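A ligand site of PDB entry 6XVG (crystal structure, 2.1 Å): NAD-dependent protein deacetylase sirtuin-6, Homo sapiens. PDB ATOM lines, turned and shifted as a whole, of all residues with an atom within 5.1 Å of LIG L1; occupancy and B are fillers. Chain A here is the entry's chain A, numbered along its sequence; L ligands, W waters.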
ATOM      1  N   GLU A  20      37.910 -20.229   7.108  1.00  0.00           N
ATOM      2  CA  GLU A  20      36.945 -19.424   6.335  1.00  0.00           C
ATOM      3  C   GLU A  20      37.042 -19.811   4.869  1.00  0.00           C
ATOM      4  O   GLU A  20      38.140 -19.977   4.386  1.00  0.00           O
ATOM      5  CB  GLU A  20      37.196 -17.932   6.552  1.00  0.00           C
ATOM      6  CG  GLU A  20      36.906 -17.527   7.963  1.00  0.00           C
ATOM      7  CD  GLU A  20      36.973 -16.032   8.233  1.00  0.00           C
ATOM      8  OE1 GLU A  20      37.767 -15.364   7.551  1.00  0.00           O
ATOM      9  OE2 GLU A  20      36.177 -15.564   9.121  1.00  0.00           O
ATOM     10  N   GLY A  50      23.397 -14.428  13.732  1.00  0.00           N
ATOM     11  CA  GLY A  50      24.357 -14.610  14.826  1.00  0.00           C
ATOM     12  C   GLY A  50      25.477 -13.612  14.730  1.00  0.00           C
ATOM     13  O   GLY A  50      25.361 -12.640  13.924  1.00  0.00           O
ATOM     14  N   ALA A  51      26.550 -13.847  15.478  1.00  0.00           N
ATOM     15  CA  ALA A  51      27.568 -12.817  15.813  1.00  0.00           C
ATOM     16  C   ALA A  51      28.296 -12.335  14.538  1.00  0.00           C
ATOM     17  O   ALA A  51      28.900 -11.254  14.579  1.00  0.00           O
ATOM     18  CB  ALA A  51      28.514 -13.378  16.839  1.00  0.00           C
ATOM     19  N   GLY A  52      28.214 -13.086  13.452  1.00  0.00           N
ATOM     20  CA  GLY A  52      28.908 -12.756  12.198  1.00  0.00           C
ATOM     21  C   GLY A  52      28.337 -11.516  11.515  1.00  0.00           C
ATOM     22  O   GLY A  52      29.051 -10.920  10.671  1.00  0.00           O
ATOM     23  N   THR A  55      30.395  -8.375  13.169  1.00  0.00           N
ATOM     24  CA  THR A  55      31.875  -8.288  13.089  1.00  0.00           C
ATOM     25  C   THR A  55      32.264  -7.029  12.301  1.00  0.00           C
ATOM     26  O   THR A  55      33.245  -6.402  12.700  1.00  0.00           O
ATOM     27  CB  THR A  55      32.499  -9.576  12.539  1.00  0.00           C
ATOM     28  OG1 THR A  55      31.946  -9.904  11.263  1.00  0.00           O
ATOM     29  CG2 THR A  55      32.330 -10.712  13.541  1.00  0.00           C
ATOM     30  N   ASP A  61      33.032 -12.194  16.958  1.00  0.00           N
ATOM     31  CA  ASP A  61      32.189 -13.416  17.027  1.00  0.00           C
ATOM     32  C   ASP A  61      32.771 -14.343  18.096  1.00  0.00           C
ATOM     33  O   ASP A  61      33.657 -13.887  18.840  1.00  0.00           O
ATOM     34  CB  ASP A  61      31.994 -14.033  15.633  1.00  0.00           C
ATOM     35  CG  ASP A  61      33.256 -14.499  14.951  1.00  0.00           C
ATOM     36  OD1 ASP A  61      34.236 -14.745  15.648  1.00  0.00           O
ATOM     37  OD2 ASP A  61      33.254 -14.606  13.708  1.00  0.00           O
ATOM     38  N   PHE A  62      32.285 -15.586  18.197  1.00  0.00           N
ATOM     39  CA  PHE A  62      32.726 -16.557  19.237  1.00  0.00           C
ATOM     40  C   PHE A  62      33.740 -17.560  18.675  1.00  0.00           C
ATOM     41  O   PHE A  62      34.720 -17.823  19.376  1.00  0.00           O
ATOM     42  CB  PHE A  62      31.515 -17.258  19.872  1.00  0.00           C
ATOM     43  CG  PHE A  62      30.697 -16.326  20.716  1.00  0.00           C
ATOM     44  CD1 PHE A  62      31.028 -16.094  22.036  1.00  0.00           C
ATOM     45  CD2 PHE A  62      29.623 -15.619  20.175  1.00  0.00           C
ATOM     46  CE1 PHE A  62      30.323 -15.191  22.810  1.00  0.00           C
ATOM     47  CE2 PHE A  62      28.923 -14.694  20.939  1.00  0.00           C
ATOM     48  CZ  PHE A  62      29.256 -14.504  22.261  1.00  0.00           C
ATOM     49  N   ARG A  63      33.502 -18.066  17.457  1.00  0.00           N
ATOM     50  CA  ARG A  63      34.212 -19.238  16.899  1.00  0.00           C
ATOM     51  C   ARG A  63      34.930 -18.877  15.595  1.00  0.00           C
ATOM     52  O   ARG A  63      35.499 -19.778  14.982  1.00  0.00           O
ATOM     53  CB  ARG A  63      33.223 -20.375  16.685  1.00  0.00           C
ATOM     54  CG  ARG A  63      32.610 -20.887  17.982  1.00  0.00           C
ATOM     55  CD  ARG A  63      31.423 -21.827  17.813  1.00  0.00           C
ATOM     56  NE  ARG A  63      30.821 -21.939  19.139  1.00  0.00           N
ATOM     57  CZ  ARG A  63      29.887 -21.159  19.670  1.00  0.00           C
ATOM     58  NH1 ARG A  63      29.294 -20.225  18.956  1.00  0.00           N
ATOM     59  NH2 ARG A  63      29.500 -21.369  20.915  1.00  0.00           N
ATOM     60  N   GLY A  64      34.911 -17.612  15.170  1.00  0.00           N
ATOM     61  CA  GLY A  64      35.680 -17.191  13.980  1.00  0.00           C
ATOM     62  C   GLY A  64      37.170 -17.208  14.307  1.00  0.00           C
ATOM     63  O   GLY A  64      37.551 -17.412  15.458  1.00  0.00           O
ATOM     64  N   TRP A  69      36.097 -17.437  21.834  1.00  0.00           N
ATOM     65  CA  TRP A  69      36.566 -18.791  22.235  1.00  0.00           C
ATOM     66  C   TRP A  69      37.877 -19.128  21.512  1.00  0.00           C
ATOM     67  O   TRP A  69      38.825 -19.634  22.171  1.00  0.00           O
ATOM     68  CB  TRP A  69      35.495 -19.865  21.978  1.00  0.00           C
ATOM     69  CG  TRP A  69      34.157 -19.650  22.596  1.00  0.00           C
ATOM     70  CD1 TRP A  69      32.954 -20.004  22.047  1.00  0.00           C
ATOM     71  CD2 TRP A  69      33.847 -19.036  23.861  1.00  0.00           C
ATOM     72  NE1 TRP A  69      31.930 -19.693  22.897  1.00  0.00           N
ATOM     73  CE2 TRP A  69      32.438 -19.096  24.017  1.00  0.00           C
ATOM     74  CE3 TRP A  69      34.602 -18.481  24.899  1.00  0.00           C
ATOM     75  CZ2 TRP A  69      31.780 -18.584  25.132  1.00  0.00           C
ATOM     76  CZ3 TRP A  69      33.951 -17.972  26.001  1.00  0.00           C
ATOM     77  CH2 TRP A  69      32.555 -18.027  26.123  1.00  0.00           C
ATOM     78  N   GLN A 111      20.458 -14.714  17.795  1.00  0.00           N
ATOM     79  CA  GLN A 111      21.222 -15.216  18.960  1.00  0.00           C
ATOM     80  C   GLN A 111      22.045 -14.083  19.568  1.00  0.00           C
ATOM     81  O   GLN A 111      22.652 -14.332  20.609  1.00  0.00           O
ATOM     82  CB  GLN A 111      22.089 -16.374  18.480  1.00  0.00           C
ATOM     83  CG  GLN A 111      21.275 -17.515  17.912  1.00  0.00           C
ATOM     84  CD  GLN A 111      22.168 -18.560  17.274  1.00  0.00           C
ATOM     85  OE1 GLN A 111      22.946 -19.205  17.965  1.00  0.00           O
ATOM     86  NE2 GLN A 111      22.067 -18.706  15.967  1.00  0.00           N
ATOM     87  N   ASN A 112      22.081 -12.903  18.953  1.00  0.00           N
ATOM     88  CA  ASN A 112      22.999 -11.811  19.367  1.00  0.00           C
ATOM     89  C   ASN A 112      22.427 -11.088  20.577  1.00  0.00           C
ATOM     90  O   ASN A 112      21.196 -10.796  20.596  1.00  0.00           O
ATOM     91  CB  ASN A 112      23.248 -10.811  18.250  1.00  0.00           C
ATOM     92  CG  ASN A 112      23.900 -11.417  17.044  1.00  0.00           C
ATOM     93  OD1 ASN A 112      24.468 -12.500  17.139  1.00  0.00           O
ATOM     94  ND2 ASN A 112      23.802 -10.745  15.898  1.00  0.00           N
ATOM     95  N   HIS A 131      18.892 -15.226  23.177  1.00  0.00           N
ATOM     96  CA  HIS A 131      19.948 -15.238  24.216  1.00  0.00           C
ATOM     97  C   HIS A 131      19.934 -13.939  25.025  1.00  0.00           C
ATOM     98  O   HIS A 131      20.828 -13.769  25.867  1.00  0.00           O
ATOM     99  CB  HIS A 131      21.311 -15.554  23.592  1.00  0.00           C
ATOM    100  CG  HIS A 131      21.342 -16.844  22.864  1.00  0.00           C
ATOM    101  ND1 HIS A 131      22.365 -17.166  21.966  1.00  0.00           N
ATOM    102  CD2 HIS A 131      20.482 -17.890  22.853  1.00  0.00           C
ATOM    103  CE1 HIS A 131      22.120 -18.353  21.432  1.00  0.00           C
ATOM    104  NE2 HIS A 131      20.967 -18.819  21.967  1.00  0.00           N
ATOM    105  N   GLY A 212      25.626 -15.278   9.325  1.00  0.00           N
ATOM    106  CA  GLY A 212      26.702 -15.103  10.318  1.00  0.00           C
ATOM    107  C   GLY A 212      26.433 -15.874  11.600  1.00  0.00           C
ATOM    108  O   GLY A 212      26.757 -15.336  12.661  1.00  0.00           O
ATOM    109  N   THR A 213      25.904 -17.086  11.496  1.00  0.00           N
ATOM    110  CA  THR A 213      25.830 -18.050  12.624  1.00  0.00           C
ATOM    111  C   THR A 213      26.403 -19.408  12.167  1.00  0.00           C
ATOM    112  O   THR A 213      26.155 -19.826  11.016  1.00  0.00           O
ATOM    113  CB  THR A 213      24.414 -18.173  13.186  1.00  0.00           C
ATOM    114  OG1 THR A 213      24.460 -19.183  14.200  1.00  0.00           O
ATOM    115  CG2 THR A 213      23.374 -18.523  12.150  1.00  0.00           C
ATOM    116  N   SER A 214      27.151 -20.055  13.074  1.00  0.00           N
ATOM    117  CA  SER A 214      27.753 -21.406  12.913  1.00  0.00           C
ATOM    118  C   SER A 214      26.705 -22.482  13.190  1.00  0.00           C
ATOM    119  O   SER A 214      26.967 -23.648  12.856  1.00  0.00           O
ATOM    120  CB  SER A 214      28.968 -21.567  13.791  1.00  0.00           C
ATOM    121  OG  SER A 214      28.622 -21.384  15.152  1.00  0.00           O
ATOM    122  N   LEU A 215      25.550 -22.111  13.772  1.00  0.00           N
ATOM    123  CA  LEU A 215      24.395 -22.997  14.071  1.00  0.00           C
ATOM    124  C   LEU A 215      24.805 -24.120  15.027  1.00  0.00           C
ATOM    125  O   LEU A 215      24.137 -25.155  15.022  1.00  0.00           O
ATOM    126  CB  LEU A 215      23.845 -23.564  12.764  1.00  0.00           C
ATOM    127  CG  LEU A 215      23.324 -22.517  11.787  1.00  0.00           C
ATOM    128  CD1 LEU A 215      22.968 -23.151  10.455  1.00  0.00           C
ATOM    129  CD2 LEU A 215      22.146 -21.766  12.375  1.00  0.00           C
ATOM    130  N   ILE A 217      24.933 -23.875  18.434  1.00  0.00           N
ATOM    131  CA  ILE A 217      24.259 -23.804  19.747  1.00  0.00           C
ATOM    132  C   ILE A 217      22.784 -24.184  19.571  1.00  0.00           C
ATOM    133  O   ILE A 217      22.104 -23.609  18.718  1.00  0.00           O
ATOM    134  CB  ILE A 217      24.449 -22.431  20.401  1.00  0.00           C
ATOM    135  CG1 ILE A 217      25.928 -22.113  20.618  1.00  0.00           C
ATOM    136  CG2 ILE A 217      23.646 -22.340  21.703  1.00  0.00           C
ATOM    137  CD1 ILE A 217      26.642 -23.059  21.576  1.00  0.00           C
ATOM    138  N   VAL A 237      24.285 -18.429   4.940  1.00  0.00           N
ATOM    139  CA  VAL A 237      25.335 -17.449   4.560  1.00  0.00           C
ATOM    140  C   VAL A 237      26.307 -17.396   5.736  1.00  0.00           C
ATOM    141  O   VAL A 237      25.878 -17.053   6.866  1.00  0.00           O
ATOM    142  CB  VAL A 237      24.746 -16.063   4.242  1.00  0.00           C
ATOM    143  CG1 VAL A 237      25.829 -15.092   3.767  1.00  0.00           C
ATOM    144  CG2 VAL A 237      23.645 -16.148   3.206  1.00  0.00           C
ATOM    145  N   ASN A 238      27.570 -17.755   5.477  1.00  0.00           N
ATOM    146  CA  ASN A 238      28.591 -17.904   6.548  1.00  0.00           C
ATOM    147  C   ASN A 238      29.957 -18.133   5.916  1.00  0.00           C
ATOM    148  O   ASN A 238      30.032 -18.845   4.910  1.00  0.00           O
ATOM    149  CB  ASN A 238      28.252 -19.057   7.490  1.00  0.00           C
ATOM    150  CG  ASN A 238      28.747 -18.791   8.896  1.00  0.00           C
ATOM    151  OD1 ASN A 238      28.290 -17.837   9.527  1.00  0.00           O
ATOM    152  ND2 ASN A 238      29.669 -19.628   9.371  1.00  0.00           N
ATOM    153  N   LEU A 239      30.995 -17.550   6.489  1.00  0.00           N
ATOM    154  CA  LEU A 239      32.391 -17.721   6.018  1.00  0.00           C
ATOM    155  C   LEU A 239      32.891 -19.116   6.437  1.00  0.00           C
ATOM    156  O   LEU A 239      33.471 -19.810   5.573  1.00  0.00           O
ATOM    157  CB  LEU A 239      33.250 -16.604   6.600  1.00  0.00           C
ATOM    158  CG  LEU A 239      33.042 -15.224   5.979  1.00  0.00           C
ATOM    159  CD1 LEU A 239      33.852 -14.169   6.736  1.00  0.00           C
ATOM    160  CD2 LEU A 239      33.441 -15.235   4.530  1.00  0.00           C
ATOM    161  N   GLN A 240      32.647 -19.521   7.681  1.00  0.00           N
ATOM    162  CA  GLN A 240      33.012 -20.882   8.148  1.00  0.00           C
ATOM    163  C   GLN A 240      31.933 -21.873   7.720  1.00  0.00           C
ATOM    164  O   GLN A 240      30.797 -21.502   7.454  1.00  0.00           O
ATOM    165  CB  GLN A 240      33.185 -20.945   9.663  1.00  0.00           C
ATOM    166  CG  GLN A 240      34.480 -20.312  10.140  1.00  0.00           C
ATOM    167  CD  GLN A 240      34.543 -20.292  11.650  1.00  0.00           C
ATOM    168  OE1 GLN A 240      33.527 -20.259  12.331  1.00  0.00           O
ATOM    169  NE2 GLN A 240      35.769 -20.300  12.172  1.00  0.00           N
ATOM    170  N   PRO A 241      32.279 -23.175   7.619  1.00  0.00           N
ATOM    171  CA  PRO A 241      31.277 -24.246   7.558  1.00  0.00           C
ATOM    172  C   PRO A 241      30.351 -24.146   8.772  1.00  0.00           C
ATOM    173  O   PRO A 241      30.770 -23.561   9.737  1.00  0.00           O
ATOM    174  CB  PRO A 241      32.103 -25.551   7.639  1.00  0.00           C
ATOM    175  CG  PRO A 241      33.487 -25.137   7.154  1.00  0.00           C
ATOM    176  CD  PRO A 241      33.660 -23.686   7.567  1.00  0.00           C
ATOM    177  N   GLY A 254      30.698 -15.889   1.892  1.00  0.00           N
ATOM    178  CA  GLY A 254      31.089 -14.497   1.664  1.00  0.00           C
ATOM    179  C   GLY A 254      30.760 -13.660   2.872  1.00  0.00           C
ATOM    180  O   GLY A 254      30.072 -14.165   3.794  1.00  0.00           O
ATOM    181  N   TYR A 255      31.272 -12.433   2.896  1.00  0.00           N
ATOM    182  CA  TYR A 255      30.907 -11.409   3.903  1.00  0.00           C
ATOM    183  C   TYR A 255      29.430 -11.103   3.763  1.00  0.00           C
ATOM    184  O   TYR A 255      29.002 -10.803   2.623  1.00  0.00           O
ATOM    185  CB  TYR A 255      31.804 -10.192   3.751  1.00  0.00           C
ATOM    186  CG  TYR A 255      33.260 -10.456   3.995  1.00  0.00           C
ATOM    187  CD1 TYR A 255      33.737 -10.659   5.282  1.00  0.00           C
ATOM    188  CD2 TYR A 255      34.172 -10.444   2.955  1.00  0.00           C
ATOM    189  CE1 TYR A 255      35.072 -10.892   5.533  1.00  0.00           C
ATOM    190  CE2 TYR A 255      35.531 -10.608   3.190  1.00  0.00           C
ATOM    191  CZ  TYR A 255      35.981 -10.806   4.502  1.00  0.00           C
ATOM    192  OH  TYR A 255      37.287 -11.026   4.767  1.00  0.00           O
ATOM    193  N   VAL A 256      28.666 -11.213   4.857  1.00  0.00           N
ATOM    194  CA  VAL A 256      27.210 -10.955   4.862  1.00  0.00           C
ATOM    195  C   VAL A 256      26.933  -9.572   4.266  1.00  0.00           C
ATOM    196  O   VAL A 256      25.985  -9.462   3.467  1.00  0.00           O
ATOM    197  CB  VAL A 256      26.578 -11.138   6.269  1.00  0.00           C
ATOM    198  CG1 VAL A 256      26.513 -12.588   6.660  1.00  0.00           C
ATOM    199  CG2 VAL A 256      27.245 -10.317   7.349  1.00  0.00           C
HETATM  200  N1  LIG L   1      30.211 -12.527   7.056  1.00  0.00           N
HETATM  201  C1  LIG L   1      29.895 -13.831   7.093  1.00  0.00           C
HETATM  202  N2  LIG L   1      30.161 -14.733   8.036  1.00  0.00           N
HETATM  203  C2  LIG L   1      30.851 -14.165   9.042  1.00  0.00           C
HETATM  204  C3  LIG L   1      31.248 -12.860   9.142  1.00  0.00           C
HETATM  205  C4  LIG L   1      30.910 -12.007   8.086  1.00  0.00           C
HETATM  206  N3  LIG L   1      31.206 -10.705   8.096  1.00  0.00           N
HETATM  207  N4  LIG L   1      31.944 -12.640  10.332  1.00  0.00           N
HETATM  208  C5  LIG L   1      31.950 -13.823  10.906  1.00  0.00           C
HETATM  209  N5  LIG L   1      31.300 -14.787  10.170  1.00  0.00           N
HETATM  210  P1  LIG L   1      29.724 -18.027  16.128  1.00  0.00           P
HETATM  211  P2  LIG L   1      26.966 -17.528  16.799  1.00  0.00           P
HETATM  212  C6  LIG L   1      30.984 -16.162  10.577  1.00  0.00           C
HETATM  213  O1  LIG L   1      29.559 -19.443  16.555  1.00  0.00           O
HETATM  214  O2  LIG L   1      26.209 -16.235  16.901  1.00  0.00           O
HETATM  215  C7  LIG L   1      27.616 -18.288  22.077  1.00  0.00           C
HETATM  216  O3  LIG L   1      27.780 -19.240  23.104  1.00  0.00           O
HETATM  217  C8  LIG L   1      32.087 -16.939  11.291  1.00  0.00           C
HETATM  218  O4  LIG L   1      32.768 -17.607  10.263  1.00  0.00           O
HETATM  219  O5  LIG L   1      30.987 -17.273  16.420  1.00  0.00           O
HETATM  220  O6  LIG L   1      26.558 -18.554  15.776  1.00  0.00           O
HETATM  221  C9  LIG L   1      26.573 -17.167  22.292  1.00  0.00           C
HETATM  222  O7  LIG L   1      25.507 -17.470  23.172  1.00  0.00           O
HETATM  223  C10 LIG L   1      31.321 -17.876  12.234  1.00  0.00           C
HETATM  224  O8  LIG L   1      31.130 -19.180  11.698  1.00  0.00           O
HETATM  225  O9  LIG L   1      28.503 -17.153  16.666  1.00  0.00           O
HETATM  226  C11 LIG L   1      26.034 -16.921  20.878  1.00  0.00           C
HETATM  227  O10 LIG L   1      24.723 -16.373  20.722  1.00  0.00           O
HETATM  228  C12 LIG L   1      29.936 -17.226  12.371  1.00  0.00           C
HETATM  229  O11 LIG L   1      29.930 -16.066  11.505  1.00  0.00           O
HETATM  230  C13 LIG L   1      25.972 -18.360  20.393  1.00  0.00           C
HETATM  231  O12 LIG L   1      27.202 -18.952  20.883  1.00  0.00           O
HETATM  232  C14 LIG L   1      29.596 -16.818  13.778  1.00  0.00           C
HETATM  233  O13 LIG L   1      29.438 -18.020  14.552  1.00  0.00           O
HETATM  234  C15 LIG L   1      25.811 -18.563  18.907  1.00  0.00           C
HETATM  235  O14 LIG L   1      27.043 -18.197  18.231  1.00  0.00           O
HETATM  236  C1  LG2 L   2      31.953 -13.421  29.458  1.00  0.00           C
HETATM  237  C2  LG2 L   2      32.156 -13.871  28.155  1.00  0.00           C
HETATM  238  C3  LG2 L   2      32.571 -13.017  27.162  1.00  0.00           C
HETATM  239  C4  LG2 L   2      32.811 -11.690  27.490  1.00  0.00           C
HETATM  240  C5  LG2 L   2      32.586 -11.214  28.807  1.00  0.00           C
HETATM  241  C6  LG2 L   2      32.165 -12.097  29.804  1.00  0.00           C
HETATM  242  C7  LG2 L   2      32.809  -9.759  29.248  1.00  0.00           C
HETATM  243  C8  LG2 L   2      27.414 -15.579  26.763  1.00  0.00           C
HETATM  244  C9  LG2 L   2      27.885 -16.793  27.201  1.00  0.00           C
HETATM  245  C10 LG2 L   2      28.927 -16.868  28.129  1.00  0.00           C
HETATM  246  C11 LG2 L   2      29.526 -15.705  28.637  1.00  0.00           C
HETATM  247  C12 LG2 L   2      29.026 -14.481  28.172  1.00  0.00           C
HETATM  248  C13 LG2 L   2      27.985 -14.430  27.241  1.00  0.00           C
HETATM  249 CL1  LG2 L   2      27.303 -12.905  26.610  1.00  0.00          CL
HETATM  250 CL2  LG2 L   2      27.096 -18.244  26.547  1.00  0.00          CL
HETATM  251  S1  LG2 L   2      30.920 -15.860  29.847  1.00  0.00           S
HETATM  252  N1  LG2 L   2      31.485 -14.358  30.438  1.00  0.00           N
HETATM  253  O1  LG2 L   2      32.050 -16.622  29.301  1.00  0.00           O
HETATM  254  O2  LG2 L   2      30.588 -16.760  30.955  1.00  0.00           O
HETATM  255  O3  LG2 L   2      32.567  -8.776  28.516  1.00  0.00           O
HETATM  256  O4  LG2 L   2      33.228  -9.536  30.413  1.00  0.00           O
HETATM  257  S2  LG2 L   2      33.369 -10.644  26.100  1.00  0.00           S
HETATM  258  O5  LG2 L   2      34.725 -10.130  26.289  1.00  0.00           O
HETATM  259  O6  LG2 L   2      33.467 -11.420  24.848  1.00  0.00           O
HETATM  260  N2  LG2 L   2      32.220  -9.436  25.956  1.00  0.00           N
HETATM  261  C14 LG2 L   2      31.108  -9.915  25.187  1.00  0.00           C
HETATM  262  C15 LG2 L   2      31.352 -10.192  23.855  1.00  0.00           C
HETATM  263  C16 LG2 L   2      30.358 -10.650  23.050  1.00  0.00           C
HETATM  264  C17 LG2 L   2      29.109 -10.866  23.586  1.00  0.00           C
HETATM  265  C18 LG2 L   2      28.860 -10.628  24.932  1.00  0.00           C
HETATM  266  C19 LG2 L   2      29.867 -10.154  25.749  1.00  0.00           C
HETATM  267  C20 LG2 L   2      29.619  -9.856  27.223  1.00  0.00           C
HETATM  268  F1  LG2 L   2      28.108 -11.319  22.776  1.00  0.00           F
HETATM  269 BR1  LG2 L   2      30.766 -10.964  21.175  1.00  0.00          BR
HETATM  270  O   HOH W   1      24.035 -19.102  25.589  1.00  0.00           O
HETATM  271  O   HOH W   2      29.562  -8.329   9.839  1.00  0.00           O
HETATM  272  O   HOH W   3      25.569 -14.526  18.790  1.00  0.00           O
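An oxygen (O11) of LIG L1 sits close to the backbone carbonyl oxygen (O) of Gly 212 (3.5 Å). Merely in contact with LIG L1: Asp 61, Gly 50, Gly 254, Tyr 255 and Ile 217. Of the 26 residues printed, 19 come within 4 Å of LIG L1.
Water W3 lies within hydrogen-bond range of O2 of LIG L1 (2.6 Å), OD1 of Asn 112 (2.8 Å) and O of Gln 111 (3.4 Å). Water W2 lies within hydrogen-bond range of the backbone carbonyl oxygen of Gly 52, the side-chain hydroxyl of Thr 55 and a nitrogen (N3) of LIG L1.
O of Arg 63 lies within hydrogen-bond range of NE2 of Gln 240 (2.9 Å). The backbone carbonyl oxygen of Gln 111 is in hydrogen-bond range of a ring nitrogen (ND1) of His 131. The backbone carbonyl oxygen (O) of Gly 212 lies within hydrogen-bond range of the backbone NH (N) of Ala 51, at 3.2 Å. The side-chain amide oxygen of Asn 112 lies within hydrogen-bond range of the backbone NH of Ala 51 (3.0 Å). The backbone carbonyl oxygen (O) of Gly 52 sits at hydrogen-bond distance from the side-chain hydroxyl (OG1) of Thr 55 (3.1 Å). The side-chain carboxylate of Asp 61 lies within hydrogen-bond range of the backbone NH of Gly 64 (3.0 Å). N of Gly 52 is in hydrogen-bond range of O of Gly 212. N of Gly 212 is in hydrogen-bond range of O of Val 237 (3.0 Å).
O5 of LIG L1 lies within hydrogen-bond range of N of Arg 63 (2.8 Å). The guanidinium group (NH1) of Arg 63 is in salt-bridge range of an oxygen (O1) of LIG L1 (2.5 Å). N of Ser 214 sits at hydrogen-bond distance from O6 of LIG L1 (3.1 Å). OG of Ser 214 lies within hydrogen-bond range of O1 of LIG L1. The side-chain hydroxyl of Thr 213 is in hydrogen-bond range of an oxygen (O6) of LIG L1 (2.7 Å). N of Gln 240 lies close to O4 of LIG L1, at 3.2 Å. O8 of LIG L1 sits at hydrogen-bond distance from OE1 of Gln 240, 2.7 Å away. N of Phe 62 lies within hydrogen-bond range of O5 of LIG L1, at 2.8 Å. A ring nitrogen (ND1) of His 131 is in hydrogen-bond range of an oxygen (O10) of LIG L1, 2.8 Å away. ND2 of Asn 238 is in hydrogen-bond range of O8 of LIG L1 (2.8 Å). N of Ala 51 sits at hydrogen-bond distance from O2 of LIG L1 (2.8 Å). The side-chain hydroxyl (OG1) of Thr 55 lies within hydrogen-bond range of a nitrogen (N4) of LIG L1, at 2.9 Å. O of Gln 111 sits at hydrogen-bond distance from O10 of LIG L1. N of Val 256 is in hydrogen-bond range of N1 of LIG L1 (3.0 Å). N3 of LIG L1 lies close to O of Gly 52 (3.4 Å). N2 of LIG L1 lies within hydrogen-bond range of N of Leu 239 (3.3 Å).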
